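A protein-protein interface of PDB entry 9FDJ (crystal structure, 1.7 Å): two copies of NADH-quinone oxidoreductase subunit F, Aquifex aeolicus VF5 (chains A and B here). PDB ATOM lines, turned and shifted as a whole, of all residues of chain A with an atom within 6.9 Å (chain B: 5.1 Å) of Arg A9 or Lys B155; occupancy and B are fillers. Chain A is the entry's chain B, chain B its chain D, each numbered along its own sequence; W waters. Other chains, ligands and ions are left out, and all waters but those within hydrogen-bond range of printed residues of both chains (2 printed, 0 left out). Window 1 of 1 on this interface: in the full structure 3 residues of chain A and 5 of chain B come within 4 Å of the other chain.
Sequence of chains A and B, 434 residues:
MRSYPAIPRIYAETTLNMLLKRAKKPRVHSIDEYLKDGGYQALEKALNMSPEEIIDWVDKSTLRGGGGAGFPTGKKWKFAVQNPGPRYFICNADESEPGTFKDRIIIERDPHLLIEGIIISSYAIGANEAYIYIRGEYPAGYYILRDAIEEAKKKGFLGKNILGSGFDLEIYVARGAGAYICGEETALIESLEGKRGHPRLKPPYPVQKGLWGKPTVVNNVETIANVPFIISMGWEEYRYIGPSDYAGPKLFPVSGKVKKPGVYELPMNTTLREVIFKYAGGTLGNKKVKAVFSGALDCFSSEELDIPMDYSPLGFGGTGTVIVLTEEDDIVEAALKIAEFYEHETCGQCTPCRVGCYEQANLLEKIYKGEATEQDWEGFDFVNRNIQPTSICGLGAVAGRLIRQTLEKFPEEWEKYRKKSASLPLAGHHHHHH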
ATOM      1  N   ALA A   6      13.463  14.516  -4.118  1.00  0.00           N
ATOM      2  CA  ALA A   6      13.607  13.072  -4.242  1.00  0.00           C
ATOM      3  C   ALA A   6      12.949  12.571  -5.531  1.00  0.00           C
ATOM      4  O   ALA A   6      11.862  13.016  -5.901  1.00  0.00           O
ATOM      5  CB  ALA A   6      13.032  12.385  -3.023  1.00  0.00           C
ATOM      6  N   ILE A   7      13.689  11.718  -6.254  1.00  0.00           N
ATOM      7  CA  ILE A   7      13.218  11.012  -7.439  1.00  0.00           C
ATOM      8  C   ILE A   7      13.350   9.516  -7.178  1.00  0.00           C
ATOM      9  O   ILE A   7      14.394   9.086  -6.693  1.00  0.00           O
ATOM     10  CB  ILE A   7      14.070  11.315  -8.685  1.00  0.00           C
ATOM     11  CG1 ILE A   7      14.532  12.760  -8.816  1.00  0.00           C
ATOM     12  CG2 ILE A   7      13.333  10.842  -9.939  1.00  0.00           C
ATOM     13  CD1 ILE A   7      15.217  13.022 -10.143  1.00  0.00           C
ATOM     14  N   PRO A   8      12.377   8.657  -7.567  1.00  0.00           N
ATOM     15  CA  PRO A   8      12.608   7.213  -7.509  1.00  0.00           C
ATOM     16  C   PRO A   8      13.623   6.828  -8.591  1.00  0.00           C
ATOM     17  O   PRO A   8      13.720   7.489  -9.614  1.00  0.00           O
ATOM     18  CB  PRO A   8      11.231   6.602  -7.717  1.00  0.00           C
ATOM     19  CG  PRO A   8      10.467   7.654  -8.461  1.00  0.00           C
ATOM     20  CD  PRO A   8      11.032   9.017  -8.051  1.00  0.00           C
ATOM     21  N   ARG A   9      14.439   5.799  -8.320  1.00  0.00           N
ATOM     22  CA  ARG A   9      15.540   5.459  -9.213  1.00  0.00           C
ATOM     23  C   ARG A   9      15.077   4.406 -10.223  1.00  0.00           C
ATOM     24  O   ARG A   9      15.200   3.191 -10.003  1.00  0.00           O
ATOM     25  CB  ARG A   9      16.758   4.981  -8.414  1.00  0.00           C
ATOM     26  CG  ARG A   9      17.694   6.089  -7.947  1.00  0.00           C
ATOM     27  CD  ARG A   9      17.121   6.901  -6.816  1.00  0.00           C
ATOM     28  NE  ARG A   9      16.911   6.043  -5.652  1.00  0.00           N
ATOM     29  CZ  ARG A   9      16.194   6.343  -4.579  1.00  0.00           C
ATOM     30  NH1 ARG A   9      16.197   5.511  -3.554  1.00  0.00           N
ATOM     31  NH2 ARG A   9      15.495   7.467  -4.527  1.00  0.00           N
ATOM     32  N   ILE A  10      14.489   4.880 -11.311  1.00  0.00           N
ATOM     33  CA  ILE A  10      13.971   4.035 -12.376  1.00  0.00           C
ATOM     34  C   ILE A  10      15.126   3.265 -13.019  1.00  0.00           C
ATOM     35  O   ILE A  10      16.157   3.858 -13.335  1.00  0.00           O
ATOM     36  CB  ILE A  10      13.217   4.924 -13.386  1.00  0.00           C
ATOM     37  CG1 ILE A  10      11.961   5.525 -12.765  1.00  0.00           C
ATOM     38  CG2 ILE A  10      12.902   4.169 -14.685  1.00  0.00           C
ATOM     39  CD1 ILE A  10      11.333   6.656 -13.561  1.00  0.00           C
ATOM     40  N   TYR A  11      14.950   1.948 -13.195  1.00  0.00           N
ATOM     41  CA  TYR A  11      15.938   1.119 -13.861  1.00  0.00           C
ATOM     42  C   TYR A  11      16.021   1.468 -15.352  1.00  0.00           C
ATOM     43  O   TYR A  11      15.016   1.628 -16.031  1.00  0.00           O
ATOM     44  CB  TYR A  11      15.634  -0.371 -13.656  1.00  0.00           C
ATOM     45  CG  TYR A  11      16.616  -1.272 -14.398  1.00  0.00           C
ATOM     46  CD1 TYR A  11      17.955  -1.311 -14.024  1.00  0.00           C
ATOM     47  CD2 TYR A  11      16.214  -2.096 -15.438  1.00  0.00           C
ATOM     48  CE1 TYR A  11      18.871  -2.107 -14.687  1.00  0.00           C
ATOM     49  CE2 TYR A  11      17.121  -2.907 -16.108  1.00  0.00           C
ATOM     50  CZ  TYR A  11      18.452  -2.916 -15.727  1.00  0.00           C
ATOM     51  OH  TYR A  11      19.388  -3.713 -16.336  1.00  0.00           O
ATOM     52  N   ALA A  12      17.254   1.507 -15.877  1.00  0.00           N
ATOM     53  CA  ALA A  12      17.475   1.785 -17.286  1.00  0.00           C
ATOM     54  C   ALA A  12      18.583   0.879 -17.831  1.00  0.00           C
ATOM     55  O   ALA A  12      19.604   0.650 -17.174  1.00  0.00           O
ATOM     56  CB  ALA A  12      17.797   3.240 -17.464  1.00  0.00           C
ATOM     57  N   PRO A  26      21.492   6.291 -12.398  1.00  0.00           N
ATOM     58  CA  PRO A  26      20.414   7.139 -11.890  1.00  0.00           C
ATOM     59  C   PRO A  26      20.841   8.324 -11.034  1.00  0.00           C
ATOM     60  O   PRO A  26      20.583   8.350  -9.832  1.00  0.00           O
ATOM     61  CB  PRO A  26      19.611   6.122 -11.097  1.00  0.00           C
ATOM     62  CG  PRO A  26      20.666   5.240 -10.489  1.00  0.00           C
ATOM     63  CD  PRO A  26      21.620   5.029 -11.644  1.00  0.00           C
ATOM     64  N   ARG A  27      21.454   9.320 -11.692  1.00  0.00           N
ATOM     65  CA  ARG A  27      21.888  10.541 -11.027  1.00  0.00           C
ATOM     66  C   ARG A  27      22.093  11.640 -12.072  1.00  0.00           C
ATOM     67  O   ARG A  27      22.168  11.362 -13.266  1.00  0.00           O
ATOM     68  CB  ARG A  27      23.192  10.316 -10.254  1.00  0.00           C
ATOM     69  CG  ARG A  27      24.345   9.852 -11.131  1.00  0.00           C
ATOM     70  CD  ARG A  27      25.641   9.580 -10.376  1.00  0.00           C
ATOM     71  NE  ARG A  27      26.727   9.180 -11.277  1.00  0.00           N
ATOM     72  CZ  ARG A  27      27.412   9.999 -12.082  1.00  0.00           C
ATOM     73  NH1 ARG A  27      28.367   9.534 -12.872  1.00  0.00           N
ATOM     74  NH2 ARG A  27      27.109  11.280 -12.133  1.00  0.00           N
ATOM     75  N   ARG A 109      18.775  12.946 -15.749  1.00  0.00           N
ATOM     76  CA  ARG A 109      20.078  12.319 -15.584  1.00  0.00           C
ATOM     77  C   ARG A 109      21.097  12.819 -16.597  1.00  0.00           C
ATOM     78  O   ARG A 109      22.292  12.875 -16.287  1.00  0.00           O
ATOM     79  CB  ARG A 109      20.024  10.797 -15.711  1.00  0.00           C
ATOM     80  CG  ARG A 109      19.039  10.188 -14.731  1.00  0.00           C
ATOM     81  CD  ARG A 109      18.829   8.735 -15.027  1.00  0.00           C
ATOM     82  NE  ARG A 109      17.810   8.237 -14.102  1.00  0.00           N
ATOM     83  CZ  ARG A 109      17.512   6.946 -13.948  1.00  0.00           C
ATOM     84  NH1 ARG A 109      18.090   6.018 -14.686  1.00  0.00           N
ATOM     85  NH2 ARG A 109      16.630   6.614 -13.040  1.00  0.00           N
ATOM     86  N   ILE B  31      16.429  -7.138  -2.766  1.00  0.00           N
ATOM     87  CA  ILE B  31      16.329  -5.754  -2.343  1.00  0.00           C
ATOM     88  C   ILE B  31      14.878  -5.347  -2.097  1.00  0.00           C
ATOM     89  O   ILE B  31      14.628  -4.553  -1.203  1.00  0.00           O
ATOM     90  CB  ILE B  31      17.067  -4.811  -3.308  1.00  0.00           C
ATOM     91  CG1 ILE B  31      17.412  -3.506  -2.585  1.00  0.00           C
ATOM     92  CG2 ILE B  31      16.280  -4.568  -4.592  1.00  0.00           C
ATOM     93  CD1 ILE B  31      18.443  -2.656  -3.290  1.00  0.00           C
ATOM     94  N   ASP B  32      13.925  -5.893  -2.860  1.00  0.00           N
ATOM     95  CA  ASP B  32      12.523  -5.527  -2.684  1.00  0.00           C
ATOM     96  C   ASP B  32      12.031  -5.936  -1.298  1.00  0.00           C
ATOM     97  O   ASP B  32      11.371  -5.143  -0.619  1.00  0.00           O
ATOM     98  CB  ASP B  32      11.654  -6.064  -3.810  1.00  0.00           C
ATOM     99  CG  ASP B  32      11.793  -5.307  -5.126  1.00  0.00           C
ATOM    100  OD1 ASP B  32      12.376  -4.202  -5.141  1.00  0.00           O
ATOM    101  OD2 ASP B  32      11.315  -5.832  -6.138  1.00  0.00           O
ATOM    102  N   LEU B  35      13.643  -3.613   1.215  1.00  0.00           N
ATOM    103  CA  LEU B  35      13.021  -2.293   1.223  1.00  0.00           C
ATOM    104  C   LEU B  35      11.667  -2.308   1.930  1.00  0.00           C
ATOM    105  O   LEU B  35      11.326  -1.361   2.635  1.00  0.00           O
ATOM    106  CB  LEU B  35      12.910  -1.821  -0.224  1.00  0.00           C
ATOM    107  CG  LEU B  35      14.234  -1.419  -0.885  1.00  0.00           C
ATOM    108  CD1 LEU B  35      14.033  -1.302  -2.378  1.00  0.00           C
ATOM    109  CD2 LEU B  35      14.749  -0.117  -0.325  1.00  0.00           C
ATOM    110  N   GLU B 151      22.007  -4.776  -7.418  1.00  0.00           N
ATOM    111  CA  GLU B 151      20.692  -4.289  -7.009  1.00  0.00           C
ATOM    112  C   GLU B 151      20.808  -2.916  -6.330  1.00  0.00           C
ATOM    113  O   GLU B 151      20.052  -1.993  -6.635  1.00  0.00           O
ATOM    114  CB  GLU B 151      19.954  -5.220  -6.039  1.00  0.00           C
ATOM    115  CG  GLU B 151      19.567  -6.593  -6.588  1.00  0.00           C
ATOM    116  CD  GLU B 151      18.816  -7.431  -5.539  1.00  0.00           C
ATOM    117  OE1 GLU B 151      19.376  -7.867  -4.496  1.00  0.00           O
ATOM    118  OE2 GLU B 151      17.582  -7.567  -5.728  1.00  0.00           O
ATOM    119  N   ALA B 152      21.740  -2.787  -5.390  1.00  0.00           N
ATOM    120  CA  ALA B 152      21.958  -1.534  -4.682  1.00  0.00           C
ATOM    121  C   ALA B 152      22.339  -0.425  -5.671  1.00  0.00           C
ATOM    122  O   ALA B 152      21.834   0.698  -5.580  1.00  0.00           O
ATOM    123  CB  ALA B 152      23.001  -1.733  -3.613  1.00  0.00           C
ATOM    124  N   LYS B 153      23.184  -0.756  -6.660  1.00  0.00           N
ATOM    125  CA  LYS B 153      23.553   0.209  -7.693  1.00  0.00           C
ATOM    126  C   LYS B 153      22.327   0.680  -8.466  1.00  0.00           C
ATOM    127  O   LYS B 153      22.138   1.878  -8.690  1.00  0.00           O
ATOM    128  CB  LYS B 153      24.579  -0.358  -8.688  1.00  0.00           C
ATOM    129  CG  LYS B 153      25.962  -0.661  -8.109  1.00  0.00           C
ATOM    130  CD  LYS B 153      27.041  -1.019  -9.131  1.00  0.00           C
ATOM    131  CE  LYS B 153      27.503   0.210  -9.874  1.00  0.00           C
ATOM    132  NZ  LYS B 153      28.695   0.019 -10.702  1.00  0.00           N
ATOM    133  N   LYS B 154      21.463  -0.275  -8.837  1.00  0.00           N
ATOM    134  CA  LYS B 154      20.263   0.027  -9.612  1.00  0.00           C
ATOM    135  C   LYS B 154      19.344   0.994  -8.865  1.00  0.00           C
ATOM    136  O   LYS B 154      18.706   1.845  -9.497  1.00  0.00           O
ATOM    137  CB  LYS B 154      19.516  -1.252 -10.005  1.00  0.00           C
ATOM    138  CG  LYS B 154      20.336  -2.109 -10.981  1.00  0.00           C
ATOM    139  CD  LYS B 154      19.745  -3.444 -11.437  1.00  0.00           C
ATOM    140  CE  LYS B 154      20.805  -4.177 -12.225  1.00  0.00           C
ATOM    141  NZ  LYS B 154      20.237  -5.306 -12.956  1.00  0.00           N
ATOM    142  N   LYS B 155      19.286   0.862  -7.535  1.00  0.00           N
ATOM    143  CA  LYS B 155      18.406   1.675  -6.710  1.00  0.00           C
ATOM    144  C   LYS B 155      19.110   2.928  -6.202  1.00  0.00           C
ATOM    145  O   LYS B 155      18.541   3.659  -5.393  1.00  0.00           O
ATOM    146  CB  LYS B 155      17.858   0.858  -5.529  1.00  0.00           C
ATOM    147  CG  LYS B 155      17.006  -0.350  -5.900  1.00  0.00           C
ATOM    148  CD  LYS B 155      15.600   0.040  -6.309  1.00  0.00           C
ATOM    149  CE  LYS B 155      14.635  -1.096  -6.320  1.00  0.00           C
ATOM    150  NZ  LYS B 155      13.407  -0.570  -6.928  1.00  0.00           N
ATOM    151  N   GLY B 156      20.350   3.165  -6.648  1.00  0.00           N
ATOM    152  CA  GLY B 156      21.053   4.400  -6.357  1.00  0.00           C
ATOM    153  C   GLY B 156      21.633   4.481  -4.945  1.00  0.00           C
ATOM    154  O   GLY B 156      21.897   5.579  -4.464  1.00  0.00           O
ATOM    155  N   PHE B 157      21.914   3.331  -4.302  1.00  0.00           N
ATOM    156  CA  PHE B 157      22.526   3.330  -2.985  1.00  0.00           C
ATOM    157  C   PHE B 157      24.048   3.227  -3.065  1.00  0.00           C
ATOM    158  O   PHE B 157      24.698   3.370  -2.038  1.00  0.00           O
ATOM    159  CB  PHE B 157      21.931   2.174  -2.176  1.00  0.00           C
ATOM    160  CG  PHE B 157      20.436   2.291  -1.946  1.00  0.00           C
ATOM    161  CD1 PHE B 157      19.864   3.476  -1.488  1.00  0.00           C
ATOM    162  CD2 PHE B 157      19.588   1.245  -2.255  1.00  0.00           C
ATOM    163  CE1 PHE B 157      18.498   3.578  -1.285  1.00  0.00           C
ATOM    164  CE2 PHE B 157      18.222   1.357  -2.061  1.00  0.00           C
ATOM    165  CZ  PHE B 157      17.675   2.526  -1.595  1.00  0.00           C
ATOM    166  N   LEU B 163      22.305   9.417  -3.596  1.00  0.00           N
ATOM    167  CA  LEU B 163      21.103  10.126  -3.175  1.00  0.00           C
ATOM    168  C   LEU B 163      21.367  11.620  -2.986  1.00  0.00           C
ATOM    169  O   LEU B 163      20.834  12.242  -2.073  1.00  0.00           O
ATOM    170  CB  LEU B 163      20.590   9.479  -1.891  1.00  0.00           C
ATOM    171  CG  LEU B 163      20.323   7.971  -1.964  1.00  0.00           C
ATOM    172  CD1 LEU B 163      19.857   7.458  -0.613  1.00  0.00           C
ATOM    173  CD2 LEU B 163      19.316   7.615  -3.052  1.00  0.00           C
HETATM  174  O   HOH W   1      18.544   2.943 -11.890  1.00  0.00           O
HETATM  175  O   HOH W   2      14.332   0.599  -9.557  1.00  0.00           O
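The guanidinium group (NE) of Arg A9 sits at hydrogen-bond distance from the backbone carbonyl oxygen (O) of Lys B155 (2.9 Å).
The backbone carbonyl oxygen (O) of Ile A7 sits at hydrogen-bond distance from the guanidinium group (NH2) of Arg A9.
O of Ala B152 is in hydrogen-bond range of N of Phe B157 (2.9 Å).
O of Lys B154 touches O of Arg A9, at 3.8 Å.
Arg A9 touches Phe B157.
Leu B163 touches Arg A9 (CD2 to CZ, 3.7 Å).
Lys B154 touches Tyr A11.
Of the printed residues of chain B, Arg A9 touches Lys B154 (3.8 Å), Lys B155 (2.9 Å), Phe B157 (3.8 Å) and Leu B163 (3.7 Å).
Lys B155 touches one residue of chain A.
Of the printed residues of chain A, Lys B154 touches Arg A9 and Tyr A11.
Of the printed residues of chain B, Tyr A11 touches Lys B154 (3.6 Å).
Printed residues of chain A within 4 Å of Phe B157: Arg A9 (3.8 Å).
Of the printed residues of chain A, Leu B163 touches Arg A9.
Lys B153 touches none of the printed residues of chain A.
The nearest residue of chain B that does not touch Arg A9 is Gly B156 (4.1 Å).
The nearest printed residue of chain A that does not touch Phe B157 is Pro A26 (6.6 Å).
Printed residues of chain B that touch a printed residue of chain A: Lys B154, Lys B155, Phe B157 and Leu B163.
Hydrophobic or aromatic side chains of chain B that line the printed part of chain A: Phe B157 and Leu B163.
Of the 10 printed residues of chain A, 2 touch a printed residue of chain B.
Hydrophobic or aromatic side chains of chain A within 4 Å of the printed part of chain B: Tyr A11.
Among the printed residues, 5 pairs touch across the chains.
Among the printed residues, no Asp or Glu carboxylate lies within 4 Å of a Lys or Arg side-chain nitrogen of the other chain.
No position is printed for both chains.
Of the 5 pairs that touch across the chains among the printed residues, none has its exchanged pair printed and touching as well.
Water W1 bridges O of Lys B154 and O of Ile A10.
Water W2 lies within hydrogen-bond range of O of Arg A9 (2.8 Å) and NZ of Lys B155 (3.0 Å).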
